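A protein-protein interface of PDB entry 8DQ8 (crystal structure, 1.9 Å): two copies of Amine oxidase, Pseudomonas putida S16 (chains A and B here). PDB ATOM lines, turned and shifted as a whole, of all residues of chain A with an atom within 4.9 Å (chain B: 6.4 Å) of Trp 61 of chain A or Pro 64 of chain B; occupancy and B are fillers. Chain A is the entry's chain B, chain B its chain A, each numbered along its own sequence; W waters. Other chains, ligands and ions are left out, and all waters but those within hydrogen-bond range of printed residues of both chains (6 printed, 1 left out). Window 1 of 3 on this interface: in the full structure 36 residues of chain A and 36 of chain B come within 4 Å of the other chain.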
ATOM      1  N   VAL A  59      20.251 -13.555  12.262  1.00  0.00           N
ATOM      2  CA  VAL A  59      19.053 -13.911  11.513  1.00  0.00           C
ATOM      3  C   VAL A  59      18.491 -12.630  10.897  1.00  0.00           C
ATOM      4  O   VAL A  59      19.031 -11.525  11.087  1.00  0.00           O
ATOM      5  CB  VAL A  59      17.972 -14.581  12.400  1.00  0.00           C
ATOM      6  CG1 VAL A  59      18.526 -15.853  13.094  1.00  0.00           C
ATOM      7  CG2 VAL A  59      17.507 -13.590  13.470  1.00  0.00           C
ATOM      8  N   HIS A  60      17.382 -12.764  10.161  1.00  0.00           N
ATOM      9  CA  HIS A  60      16.820 -11.610   9.460  1.00  0.00           C
ATOM     10  C   HIS A  60      15.372 -11.905   9.060  1.00  0.00           C
ATOM     11  O   HIS A  60      14.981 -13.062   8.922  1.00  0.00           O
ATOM     12  CB  HIS A  60      17.646 -11.303   8.218  1.00  0.00           C
ATOM     13  CG  HIS A  60      17.469  -9.909   7.681  1.00  0.00           C
ATOM     14  ND1 HIS A  60      16.517  -9.594   6.717  1.00  0.00           N
ATOM     15  CD2 HIS A  60      18.174  -8.760   7.913  1.00  0.00           C
ATOM     16  CE1 HIS A  60      16.640  -8.316   6.393  1.00  0.00           C
ATOM     17  NE2 HIS A  60      17.645  -7.791   7.090  1.00  0.00           N
ATOM     18  N   TRP A  61      14.588 -10.839   8.883  1.00  0.00           N
ATOM     19  CA  TRP A  61      13.190 -11.018   8.534  1.00  0.00           C
ATOM     20  C   TRP A  61      13.009 -11.430   7.071  1.00  0.00           C
ATOM     21  O   TRP A  61      11.918 -11.887   6.733  1.00  0.00           O
ATOM     22  CB  TRP A  61      12.384  -9.726   8.795  1.00  0.00           C
ATOM     23  CG  TRP A  61      13.050  -8.479   8.254  1.00  0.00           C
ATOM     24  CD1 TRP A  61      12.937  -7.939   6.973  1.00  0.00           C
ATOM     25  CD2 TRP A  61      13.971  -7.623   8.979  1.00  0.00           C
ATOM     26  NE1 TRP A  61      13.740  -6.784   6.887  1.00  0.00           N
ATOM     27  CE2 TRP A  61      14.399  -6.618   8.093  1.00  0.00           C
ATOM     28  CE3 TRP A  61      14.506  -7.651  10.301  1.00  0.00           C
ATOM     29  CZ2 TRP A  61      15.308  -5.599   8.487  1.00  0.00           C
ATOM     30  CZ3 TRP A  61      15.380  -6.661  10.699  1.00  0.00           C
ATOM     31  CH2 TRP A  61      15.784  -5.620   9.776  1.00  0.00           C
ATOM     32  N   LEU A  62      14.031 -11.287   6.218  1.00  0.00           N
ATOM     33  CA  LEU A  62      13.947 -11.897   4.881  1.00  0.00           C
ATOM     34  C   LEU A  62      14.102 -13.417   4.930  1.00  0.00           C
ATOM     35  O   LEU A  62      13.934 -14.075   3.889  1.00  0.00           O
ATOM     36  CB  LEU A  62      15.036 -11.315   3.946  1.00  0.00           C
ATOM     37  CG  LEU A  62      14.786  -9.844   3.633  1.00  0.00           C
ATOM     38  CD1 LEU A  62      15.954  -9.164   2.835  1.00  0.00           C
ATOM     39  CD2 LEU A  62      13.469  -9.713   2.842  1.00  0.00           C
ATOM     40  N   GLN A  63      14.423 -13.994   6.087  1.00  0.00           N
ATOM     41  CA  GLN A  63      14.543 -15.450   6.201  1.00  0.00           C
ATOM     42  C   GLN A  63      13.207 -16.017   6.705  1.00  0.00           C
ATOM     43  O   GLN A  63      12.845 -15.845   7.901  1.00  0.00           O
ATOM     44  CB  GLN A  63      15.704 -15.822   7.156  1.00  0.00           C
ATOM     45  CG  GLN A  63      17.036 -15.328   6.570  1.00  0.00           C
ATOM     46  CD  GLN A  63      18.232 -15.495   7.565  1.00  0.00           C
ATOM     47  OE1 GLN A  63      18.024 -15.465   8.804  1.00  0.00           O
ATOM     48  NE2 GLN A  63      19.455 -15.660   7.032  1.00  0.00           N
ATOM     49  N   PRO A  64      12.409 -16.636   5.838  1.00  0.00           N
ATOM     50  CA  PRO A  64      10.977 -16.802   6.163  1.00  0.00           C
ATOM     51  C   PRO A  64      10.710 -17.766   7.318  1.00  0.00           C
ATOM     52  O   PRO A  64       9.820 -17.492   8.144  1.00  0.00           O
ATOM     53  CB  PRO A  64      10.376 -17.314   4.835  1.00  0.00           C
ATOM     54  CG  PRO A  64      11.562 -17.963   4.096  1.00  0.00           C
ATOM     55  CD  PRO A  64      12.771 -17.119   4.489  1.00  0.00           C
ATOM     56  N   TRP A  67      11.982 -16.338  10.803  1.00  0.00           N
ATOM     57  CA  TRP A  67      11.244 -15.135  11.178  1.00  0.00           C
ATOM     58  C   TRP A  67       9.829 -15.511  11.604  1.00  0.00           C
ATOM     59  O   TRP A  67       9.306 -14.971  12.586  1.00  0.00           O
ATOM     60  CB  TRP A  67      11.174 -14.122  10.032  1.00  0.00           C
ATOM     61  CG  TRP A  67      10.605 -12.789  10.497  1.00  0.00           C
ATOM     62  CD1 TRP A  67       9.311 -12.307  10.334  1.00  0.00           C
ATOM     63  CD2 TRP A  67      11.308 -11.802  11.276  1.00  0.00           C
ATOM     64  NE1 TRP A  67       9.200 -11.088  10.942  1.00  0.00           N
ATOM     65  CE2 TRP A  67      10.410 -10.749  11.528  1.00  0.00           C
ATOM     66  CE3 TRP A  67      12.595 -11.740  11.784  1.00  0.00           C
ATOM     67  CZ2 TRP A  67      10.762  -9.612  12.287  1.00  0.00           C
ATOM     68  CZ3 TRP A  67      12.980 -10.588  12.533  1.00  0.00           C
ATOM     69  CH2 TRP A  67      12.053  -9.552  12.781  1.00  0.00           C
ATOM     70  N   ALA A  68       9.179 -16.414  10.867  1.00  0.00           N
ATOM     71  CA  ALA A  68       7.845 -16.819  11.330  1.00  0.00           C
ATOM     72  C   ALA A  68       7.880 -17.382  12.756  1.00  0.00           C
ATOM     73  O   ALA A  68       6.934 -17.142  13.550  1.00  0.00           O
ATOM     74  CB  ALA A  68       7.221 -17.854  10.370  1.00  0.00           C
ATOM     75  N   VAL A  77      14.407  -8.565  17.594  1.00  0.00           N
ATOM     76  CA  VAL A  77      15.810  -8.596  17.140  1.00  0.00           C
ATOM     77  C   VAL A  77      16.662  -7.800  18.109  1.00  0.00           C
ATOM     78  O   VAL A  77      16.207  -6.851  18.748  1.00  0.00           O
ATOM     79  CB  VAL A  77      16.016  -8.057  15.707  1.00  0.00           C
ATOM     80  CG1 VAL A  77      15.291  -8.907  14.675  1.00  0.00           C
ATOM     81  CG2 VAL A  77      15.586  -6.567  15.601  1.00  0.00           C
ATOM     82  N   ASP A 197      22.859  -7.468   4.890  1.00  0.00           N
ATOM     83  CA  ASP A 197      22.103  -7.208   6.123  1.00  0.00           C
ATOM     84  C   ASP A 197      21.593  -8.502   6.769  1.00  0.00           C
ATOM     85  O   ASP A 197      21.412  -8.562   8.013  1.00  0.00           O
ATOM     86  CB  ASP A 197      20.925  -6.296   5.791  1.00  0.00           C
ATOM     87  CG  ASP A 197      20.451  -5.478   7.008  1.00  0.00           C
ATOM     88  OD1 ASP A 197      21.318  -4.910   7.691  1.00  0.00           O
ATOM     89  OD2 ASP A 197      19.216  -5.406   7.251  1.00  0.00           O
ATOM     90  N   TYR A 202      21.649  -8.855  13.027  1.00  0.00           N
ATOM     91  CA  TYR A 202      20.623  -8.935  14.079  1.00  0.00           C
ATOM     92  C   TYR A 202      20.665 -10.307  14.747  1.00  0.00           C
ATOM     93  O   TYR A 202      20.687 -11.317  14.040  1.00  0.00           O
ATOM     94  CB  TYR A 202      19.215  -8.738  13.457  1.00  0.00           C
ATOM     95  CG  TYR A 202      19.074  -7.357  12.841  1.00  0.00           C
ATOM     96  CD1 TYR A 202      18.884  -6.242  13.678  1.00  0.00           C
ATOM     97  CD2 TYR A 202      19.173  -7.173  11.466  1.00  0.00           C
ATOM     98  CE1 TYR A 202      18.767  -4.968  13.136  1.00  0.00           C
ATOM     99  CE2 TYR A 202      19.055  -5.899  10.894  1.00  0.00           C
ATOM    100  CZ  TYR A 202      18.855  -4.796  11.758  1.00  0.00           C
ATOM    101  OH  TYR A 202      18.737  -3.514  11.275  1.00  0.00           O
ATOM    102  N   HIS B  60       4.953 -14.763  -2.276  1.00  0.00           N
ATOM    103  CA  HIS B  60       6.372 -14.872  -2.615  1.00  0.00           C
ATOM    104  C   HIS B  60       7.136 -15.412  -1.414  1.00  0.00           C
ATOM    105  O   HIS B  60       6.704 -15.251  -0.269  1.00  0.00           O
ATOM    106  CB  HIS B  60       6.940 -13.492  -2.986  1.00  0.00           C
ATOM    107  CG  HIS B  60       8.206 -13.536  -3.791  1.00  0.00           C
ATOM    108  ND1 HIS B  60       9.467 -13.501  -3.201  1.00  0.00           N
ATOM    109  CD2 HIS B  60       8.418 -13.525  -5.135  1.00  0.00           C
ATOM    110  CE1 HIS B  60      10.390 -13.507  -4.150  1.00  0.00           C
ATOM    111  NE2 HIS B  60       9.783 -13.491  -5.329  1.00  0.00           N
ATOM    112  N   TRP B  61       8.298 -16.001  -1.688  1.00  0.00           N
ATOM    113  CA  TRP B  61       9.113 -16.565  -0.617  1.00  0.00           C
ATOM    114  C   TRP B  61       9.832 -15.502   0.207  1.00  0.00           C
ATOM    115  O   TRP B  61      10.319 -15.853   1.289  1.00  0.00           O
ATOM    116  CB  TRP B  61      10.169 -17.568  -1.154  1.00  0.00           C
ATOM    117  CG  TRP B  61      10.933 -17.049  -2.333  1.00  0.00           C
ATOM    118  CD1 TRP B  61      12.094 -16.295  -2.310  1.00  0.00           C
ATOM    119  CD2 TRP B  61      10.573 -17.220  -3.729  1.00  0.00           C
ATOM    120  NE1 TRP B  61      12.471 -15.989  -3.639  1.00  0.00           N
ATOM    121  CE2 TRP B  61      11.538 -16.533  -4.500  1.00  0.00           C
ATOM    122  CE3 TRP B  61       9.497 -17.864  -4.395  1.00  0.00           C
ATOM    123  CZ2 TRP B  61      11.488 -16.489  -5.894  1.00  0.00           C
ATOM    124  CZ3 TRP B  61       9.462 -17.849  -5.785  1.00  0.00           C
ATOM    125  CH2 TRP B  61      10.453 -17.139  -6.530  1.00  0.00           C
ATOM    126  N   LEU B  62       9.901 -14.246  -0.250  1.00  0.00           N
ATOM    127  CA  LEU B  62      10.402 -13.159   0.595  1.00  0.00           C
ATOM    128  C   LEU B  62       9.353 -12.736   1.627  1.00  0.00           C
ATOM    129  O   LEU B  62       9.657 -11.905   2.502  1.00  0.00           O
ATOM    130  CB  LEU B  62      10.785 -11.924  -0.255  1.00  0.00           C
ATOM    131  CG  LEU B  62      11.988 -12.177  -1.164  1.00  0.00           C
ATOM    132  CD1 LEU B  62      12.312 -10.996  -2.106  1.00  0.00           C
ATOM    133  CD2 LEU B  62      13.236 -12.453  -0.281  1.00  0.00           C
ATOM    134  N   GLN B  63       8.137 -13.277   1.553  1.00  0.00           N
ATOM    135  CA  GLN B  63       7.095 -12.959   2.536  1.00  0.00           C
ATOM    136  C   GLN B  63       7.095 -14.040   3.618  1.00  0.00           C
ATOM    137  O   GLN B  63       6.655 -15.195   3.355  1.00  0.00           O
ATOM    138  CB  GLN B  63       5.717 -12.859   1.850  1.00  0.00           C
ATOM    139  CG  GLN B  63       5.729 -11.721   0.812  1.00  0.00           C
ATOM    140  CD  GLN B  63       4.432 -11.682  -0.044  1.00  0.00           C
ATOM    141  OE1 GLN B  63       3.782 -12.730  -0.230  1.00  0.00           O
ATOM    142  NE2 GLN B  63       4.050 -10.495  -0.518  1.00  0.00           N
ATOM    143  N   PRO B  64       7.611 -13.755   4.815  1.00  0.00           N
ATOM    144  CA  PRO B  64       8.016 -14.864   5.706  1.00  0.00           C
ATOM    145  C   PRO B  64       6.838 -15.664   6.264  1.00  0.00           C
ATOM    146  O   PRO B  64       6.950 -16.906   6.411  1.00  0.00           O
ATOM    147  CB  PRO B  64       8.820 -14.142   6.818  1.00  0.00           C
ATOM    148  CG  PRO B  64       8.276 -12.716   6.812  1.00  0.00           C
ATOM    149  CD  PRO B  64       7.959 -12.420   5.351  1.00  0.00           C
ATOM    150  N   HIS B  65       5.736 -15.013   6.639  1.00  0.00           N
ATOM    151  CA  HIS B  65       4.705 -15.752   7.347  1.00  0.00           C
ATOM    152  C   HIS B  65       3.950 -16.688   6.396  1.00  0.00           C
ATOM    153  O   HIS B  65       3.772 -17.903   6.684  1.00  0.00           O
ATOM    154  CB  HIS B  65       3.762 -14.752   8.038  1.00  0.00           C
ATOM    155  CG  HIS B  65       4.542 -13.713   8.823  1.00  0.00           C
ATOM    156  ND1 HIS B  65       4.833 -12.453   8.315  1.00  0.00           N
ATOM    157  CD2 HIS B  65       5.076 -13.761  10.076  1.00  0.00           C
ATOM    158  CE1 HIS B  65       5.563 -11.790   9.222  1.00  0.00           C
ATOM    159  NE2 HIS B  65       5.689 -12.546  10.305  1.00  0.00           N
ATOM    160  N   VAL B  66       3.539 -16.162   5.234  1.00  0.00           N
ATOM    161  CA  VAL B  66       2.804 -17.038   4.309  1.00  0.00           C
ATOM    162  C   VAL B  66       3.723 -18.097   3.730  1.00  0.00           C
ATOM    163  O   VAL B  66       3.307 -19.252   3.519  1.00  0.00           O
ATOM    164  CB  VAL B  66       2.084 -16.209   3.204  1.00  0.00           C
ATOM    165  CG1 VAL B  66       3.106 -15.509   2.259  1.00  0.00           C
ATOM    166  CG2 VAL B  66       1.160 -17.120   2.347  1.00  0.00           C
ATOM    167  N   TRP B  67       4.997 -17.752   3.468  1.00  0.00           N
ATOM    168  CA  TRP B  67       5.885 -18.786   2.953  1.00  0.00           C
ATOM    169  C   TRP B  67       6.075 -19.901   3.981  1.00  0.00           C
ATOM    170  O   TRP B  67       6.098 -21.086   3.623  1.00  0.00           O
ATOM    171  CB  TRP B  67       7.252 -18.214   2.548  1.00  0.00           C
ATOM    172  CG  TRP B  67       8.074 -19.238   1.758  1.00  0.00           C
ATOM    173  CD1 TRP B  67       9.112 -20.030   2.214  1.00  0.00           C
ATOM    174  CD2 TRP B  67       7.878 -19.595   0.378  1.00  0.00           C
ATOM    175  NE1 TRP B  67       9.550 -20.840   1.209  1.00  0.00           N
ATOM    176  CE2 TRP B  67       8.825 -20.597   0.064  1.00  0.00           C
ATOM    177  CE3 TRP B  67       6.956 -19.210  -0.583  1.00  0.00           C
ATOM    178  CZ2 TRP B  67       8.896 -21.212  -1.196  1.00  0.00           C
ATOM    179  CZ3 TRP B  67       7.049 -19.794  -1.883  1.00  0.00           C
ATOM    180  CH2 TRP B  67       7.999 -20.805  -2.152  1.00  0.00           C
ATOM    181  N   ALA B  68       6.285 -19.549   5.256  1.00  0.00           N
ATOM    182  CA  ALA B  68       6.423 -20.627   6.234  1.00  0.00           C
ATOM    183  C   ALA B  68       5.188 -21.542   6.244  1.00  0.00           C
ATOM    184  O   ALA B  68       5.311 -22.778   6.431  1.00  0.00           O
ATOM    185  CB  ALA B  68       6.682 -20.045   7.633  1.00  0.00           C
ATOM    186  N   GLU B  69       3.982 -20.963   6.088  1.00  0.00           N
ATOM    187  CA  GLU B  69       2.784 -21.824   6.027  1.00  0.00           C
ATOM    188  C   GLU B  69       2.817 -22.742   4.795  1.00  0.00           C
ATOM    189  O   GLU B  69       2.407 -23.917   4.847  1.00  0.00           O
ATOM    190  CB  GLU B  69       1.495 -20.965   5.985  1.00  0.00           C
ATOM    191  CG  GLU B  69       1.353 -20.090   7.255  1.00  0.00           C
ATOM    192  CD  GLU B  69       1.309 -20.898   8.531  1.00  0.00           C
ATOM    193  OE1 GLU B  69       1.053 -22.143   8.501  1.00  0.00           O
ATOM    194  OE2 GLU B  69       1.494 -20.286   9.608  1.00  0.00           O
ATOM    195  N   PHE B 124      13.449   3.090   6.591  1.00  0.00           N
ATOM    196  CA  PHE B 124      12.969   1.791   7.070  1.00  0.00           C
ATOM    197  C   PHE B 124      14.107   0.778   7.071  1.00  0.00           C
ATOM    198  O   PHE B 124      14.073  -0.221   6.335  1.00  0.00           O
ATOM    199  CB  PHE B 124      11.803   1.287   6.206  1.00  0.00           C
ATOM    200  CG  PHE B 124      10.517   2.089   6.415  1.00  0.00           C
ATOM    201  CD1 PHE B 124       9.766   1.907   7.596  1.00  0.00           C
ATOM    202  CD2 PHE B 124      10.114   3.027   5.503  1.00  0.00           C
ATOM    203  CE1 PHE B 124       8.609   2.677   7.844  1.00  0.00           C
ATOM    204  CE2 PHE B 124       8.954   3.786   5.709  1.00  0.00           C
ATOM    205  CZ  PHE B 124       8.194   3.626   6.888  1.00  0.00           C
ATOM    206  N   PRO B 125      15.079   0.945   7.940  1.00  0.00           N
ATOM    207  CA  PRO B 125      16.058  -0.150   8.137  1.00  0.00           C
ATOM    208  C   PRO B 125      15.425  -1.367   8.766  1.00  0.00           C
ATOM    209  O   PRO B 125      15.997  -2.450   8.649  1.00  0.00           O
ATOM    210  CB  PRO B 125      17.124   0.469   9.079  1.00  0.00           C
ATOM    211  CG  PRO B 125      16.347   1.603   9.804  1.00  0.00           C
ATOM    212  CD  PRO B 125      15.304   2.108   8.828  1.00  0.00           C
ATOM    213  N   ARG B 126      14.275  -1.209   9.456  1.00  0.00           N
ATOM    214  CA  ARG B 126      13.611  -2.307  10.171  1.00  0.00           C
ATOM    215  C   ARG B 126      12.153  -2.228   9.798  1.00  0.00           C
ATOM    216  O   ARG B 126      11.349  -1.670  10.562  1.00  0.00           O
ATOM    217  CB  ARG B 126      13.759  -2.169  11.711  1.00  0.00           C
ATOM    218  CG  ARG B 126      15.138  -2.263  12.246  1.00  0.00           C
ATOM    219  CD  ARG B 126      15.012  -2.470  13.787  1.00  0.00           C
ATOM    220  NE  ARG B 126      16.278  -2.243  14.486  1.00  0.00           N
ATOM    221  CZ  ARG B 126      16.428  -2.494  15.785  1.00  0.00           C
ATOM    222  NH1 ARG B 126      15.422  -2.971  16.525  1.00  0.00           N
ATOM    223  NH2 ARG B 126      17.596  -2.216  16.366  1.00  0.00           N
ATOM    224  N   PRO B 127      11.776  -2.705   8.597  1.00  0.00           N
ATOM    225  CA  PRO B 127      10.370  -2.528   8.137  1.00  0.00           C
ATOM    226  C   PRO B 127       9.320  -3.132   9.064  1.00  0.00           C
ATOM    227  O   PRO B 127       8.149  -2.707   9.015  1.00  0.00           O
ATOM    228  CB  PRO B 127      10.362  -3.216   6.769  1.00  0.00           C
ATOM    229  CG  PRO B 127      11.600  -4.042   6.693  1.00  0.00           C
ATOM    230  CD  PRO B 127      12.633  -3.341   7.584  1.00  0.00           C
ATOM    231  N   HIS B 128       9.672  -4.132   9.899  1.00  0.00           N
ATOM    232  CA  HIS B 128       8.673  -4.644  10.852  1.00  0.00           C
ATOM    233  C   HIS B 128       8.566  -3.803  12.104  1.00  0.00           C
ATOM    234  O   HIS B 128       7.823  -4.172  13.028  1.00  0.00           O
ATOM    235  CB  HIS B 128       9.006  -6.099  11.207  1.00  0.00           C
ATOM    236  CG  HIS B 128       8.832  -7.017  10.045  1.00  0.00           C
ATOM    237  ND1 HIS B 128       7.603  -7.577   9.715  1.00  0.00           N
ATOM    238  CD2 HIS B 128       9.708  -7.429   9.096  1.00  0.00           C
ATOM    239  CE1 HIS B 128       7.751  -8.302   8.615  1.00  0.00           C
ATOM    240  NE2 HIS B 128       9.003  -8.211   8.201  1.00  0.00           N
ATOM    241  N   GLU B 129       9.308  -2.693  12.189  1.00  0.00           N
ATOM    242  CA  GLU B 129       9.137  -1.697  13.264  1.00  0.00           C
ATOM    243  C   GLU B 129       8.928  -0.361  12.576  1.00  0.00           C
ATOM    244  O   GLU B 129       9.866   0.446  12.448  1.00  0.00           O
ATOM    245  CB  GLU B 129      10.336  -1.675  14.226  1.00  0.00           C
ATOM    246  CG  GLU B 129      10.598  -2.999  14.886  1.00  0.00           C
ATOM    247  CD  GLU B 129      11.832  -2.955  15.812  1.00  0.00           C
ATOM    248  OE1 GLU B 129      11.957  -2.004  16.647  1.00  0.00           O
ATOM    249  OE2 GLU B 129      12.703  -3.838  15.655  1.00  0.00           O
ATOM    250  N   ALA B 186      10.833  -1.649   1.337  1.00  0.00           N
ATOM    251  CA  ALA B 186      11.832  -2.205   2.259  1.00  0.00           C
ATOM    252  C   ALA B 186      11.564  -3.686   2.552  1.00  0.00           C
ATOM    253  O   ALA B 186      12.489  -4.505   2.561  1.00  0.00           O
ATOM    254  CB  ALA B 186      11.814  -1.389   3.598  1.00  0.00           C
ATOM    255  N   CYS B 187      10.297  -4.059   2.773  1.00  0.00           N
ATOM    256  CA  CYS B 187       9.989  -5.471   3.001  1.00  0.00           C
ATOM    257  C   CYS B 187      10.463  -6.345   1.822  1.00  0.00           C
ATOM    258  O   CYS B 187      10.870  -7.491   2.016  1.00  0.00           O
ATOM    259  CB  CYS B 187       8.474  -5.657   3.161  1.00  0.00           C
ATOM    260  SG  CYS B 187       7.840  -5.109   4.811  1.00  0.00           S
ATOM    261  N   TRP B 190      14.404  -3.859  -0.304  1.00  0.00           N
ATOM    262  CA  TRP B 190      14.873  -2.516  -0.662  1.00  0.00           C
ATOM    263  C   TRP B 190      15.322  -2.420  -2.122  1.00  0.00           C
ATOM    264  O   TRP B 190      16.281  -1.709  -2.458  1.00  0.00           O
ATOM    265  CB  TRP B 190      16.041  -2.090   0.255  1.00  0.00           C
ATOM    266  CG  TRP B 190      15.797  -2.042   1.745  1.00  0.00           C
ATOM    267  CD1 TRP B 190      15.256  -1.020   2.469  1.00  0.00           C
ATOM    268  CD2 TRP B 190      16.156  -3.061   2.695  1.00  0.00           C
ATOM    269  NE1 TRP B 190      15.252  -1.338   3.829  1.00  0.00           N
ATOM    270  CE2 TRP B 190      15.802  -2.582   3.982  1.00  0.00           C
ATOM    271  CE3 TRP B 190      16.781  -4.313   2.578  1.00  0.00           C
ATOM    272  CZ2 TRP B 190      16.051  -3.298   5.137  1.00  0.00           C
ATOM    273  CZ3 TRP B 190      17.032  -5.058   3.755  1.00  0.00           C
ATOM    274  CH2 TRP B 190      16.677  -4.532   5.018  1.00  0.00           C
ATOM    275  N   TRP B 409       3.998  -6.700   5.711  1.00  0.00           N
ATOM    276  CA  TRP B 409       3.279  -6.741   4.434  1.00  0.00           C
ATOM    277  C   TRP B 409       1.784  -6.454   4.648  1.00  0.00           C
ATOM    278  O   TRP B 409       0.928  -7.331   4.534  1.00  0.00           O
ATOM    279  CB  TRP B 409       3.485  -8.118   3.814  1.00  0.00           C
ATOM    280  CG  TRP B 409       4.896  -8.408   3.318  1.00  0.00           C
ATOM    281  CD1 TRP B 409       5.916  -9.047   3.996  1.00  0.00           C
ATOM    282  CD2 TRP B 409       5.420  -8.053   2.025  1.00  0.00           C
ATOM    283  NE1 TRP B 409       7.076  -9.098   3.167  1.00  0.00           N
ATOM    284  CE2 TRP B 409       6.773  -8.477   1.974  1.00  0.00           C
ATOM    285  CE3 TRP B 409       4.877  -7.347   0.918  1.00  0.00           C
ATOM    286  CZ2 TRP B 409       7.588  -8.278   0.848  1.00  0.00           C
ATOM    287  CZ3 TRP B 409       5.700  -7.150  -0.191  1.00  0.00           C
ATOM    288  CH2 TRP B 409       7.032  -7.621  -0.216  1.00  0.00           C
ATOM    289  N   ASP B 414       0.256 -12.102   3.462  1.00  0.00           N
ATOM    290  CA  ASP B 414       1.280 -12.291   4.497  1.00  0.00           C
ATOM    291  C   ASP B 414       1.002 -11.488   5.765  1.00  0.00           C
ATOM    292  O   ASP B 414       1.200 -12.002   6.886  1.00  0.00           O
ATOM    293  CB  ASP B 414       2.655 -11.908   3.946  1.00  0.00           C
ATOM    294  CG  ASP B 414       3.758 -12.255   4.955  1.00  0.00           C
ATOM    295  OD1 ASP B 414       4.210 -13.433   4.956  1.00  0.00           O
ATOM    296  OD2 ASP B 414       4.089 -11.340   5.766  1.00  0.00           O
HETATM  297  O   HOH W   1      18.389  -1.055  12.749  1.00  0.00           O
HETATM  298  O   HOH W   2      18.581  -3.165   8.707  1.00  0.00           O
HETATM  299  O   HOH W   3      13.953  -6.176   4.032  1.00  0.00           O
HETATM  300  O   HOH W   4      12.566  -6.185  17.498  1.00  0.00           O
HETATM  301  O   HOH W   5      10.041  -9.765   6.151  1.00  0.00           O
HETATM  302  O   HOH W   6      16.211  -4.037  19.153  1.00  0.00           O
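Water W2 lies within hydrogen-bond range of the side-chain hydroxyl of Tyr 202 of chain A (2.6 Å), the backbone carbonyl oxygen of Pro 125 of chain B (2.7 Å) and the side-chain carboxylate of Asp 197 of chain A (2.7 Å).
Water W5 lies within hydrogen-bond range of a ring nitrogen (NE2) of His 128 of chain B (2.8 Å) and the backbone carbonyl oxygen of Trp 61 of chain A (2.9 Å).
Water W6 bridges O of Val 77 of chain A and NH1 of Arg 126 of chain B.
Water W1 lies within hydrogen-bond range of OH of Tyr 202 of chain A (2.9 Å) and NE of Arg 126 of chain B (3.0 Å).
Trp 61 of chain A touches Pro 64 of chain B, and with the chains exchanged Pro 64 of chain A touches Trp 61 of chain B.
Pro 64 of chain B touches its own counterpart, Pro 64 of chain A.
Pro 64 of chain A touches Trp 67 of chain B, and with the chains exchanged Trp 67 of chain A touches Pro 64 of chain B.
Ala 68 of chain A touches its own counterpart, Ala 68 of chain B.
Of the 20 pairs that touch across the chains among the printed residues, 6 have their exchanged pair printed and touching as well.
The backbone carbonyl oxygen (O) of Pro 64 of chain B lies close to the backbone carbonyl oxygen (O) of Pro 64 of chain A (3.4 Å).
O of Trp 61 of chain A touches CG of Pro 64 of chain B (3.7 Å).
Pro 127 of chain B touches Trp 61 of chain A.
CZ2 of Trp 61 of chain A touches CH2 of Trp 190 of chain B, 3.9 Å away.
Trp 61 of chain B touches Pro 64 of chain A (O to CG, 3.7 Å).
CD1 of Trp 67 of chain A touches CG of Pro 64 of chain B, at 3.7 Å.
His 65 of chain B touches Trp 67 of chain A.
His 128 of chain B touches Trp 67 of chain A.
CB of Ala 68 of chain A touches CB of Ala 68 of chain B (3.5 Å).
Glu 129 of chain B touches Val 77 of chain A (OE2 to CG2, 3.97 Å).
Asp 197 of chain A touches Trp 190 of chain B (OD2 to CH2, 3.5 Å).
Of the 11 printed residues of chain A, 9 touch a printed residue of chain B.
Hydrophobic or aromatic side chains of chain A that line the printed part of chain B: His 60, Trp 61, Leu 62, Pro 64, Trp 67, Ala 68, Val 77 and Tyr 202.
Of the 21 printed residues of chain B, 12 touch a printed residue of chain A.
ND1 of His 60 of chain A sits at hydrogen-bond distance from N of Leu 62 of chain A (3.0 Å).
O of Phe 124 of chain B sits at hydrogen-bond distance from NE1 of Trp 190 of chain B.
The backbone carbonyl oxygen of Tyr 202 of chain A lies within hydrogen-bond range of the backbone NH of Val 59 of chain A (2.9 Å).
The side-chain carboxylate (OD1) of Asp 414 of chain B lies within hydrogen-bond range of the backbone NH (N) of His 65 of chain B (2.8 Å).
The backbone NH (N) of His 60 of chain A is in hydrogen-bond range of the side-chain amide oxygen (OE1) of Gln 63 of chain A, at 3.1 Å.
Val 59 of chain A touches none of the printed residues of chain B.
Of the printed residues of chain B, Trp 61 of chain A touches Pro 64 (3.7 Å), Pro 125 (3.2 Å), Arg 126 (3.98 Å), Pro 127 (3.5 Å), His 128 (3.5 Å) and Trp 190 (3.9 Å).
Of the printed residues of chain B, Val 77 of chain A touches Arg 126 (3.7 Å) and Glu 129 (3.97 Å).
Pro 64 of chain B touches three residues of chain A.
Printed residues of chain A within 4 Å of His 65 of chain B: Trp 67 (3.6 Å).
Printed residues of chain A within 4 Å of Ala 68 of chain B: Ala 68.
Glu 69 of chain B touches none of the printed residues of chain A.
Of the printed residues of chain A, His 128 of chain B touches Trp 61 and Trp 67.
The nearest residue of chain A that does not touch Pro 64 of chain B is Ala 68 of chain A (4.1 Å).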
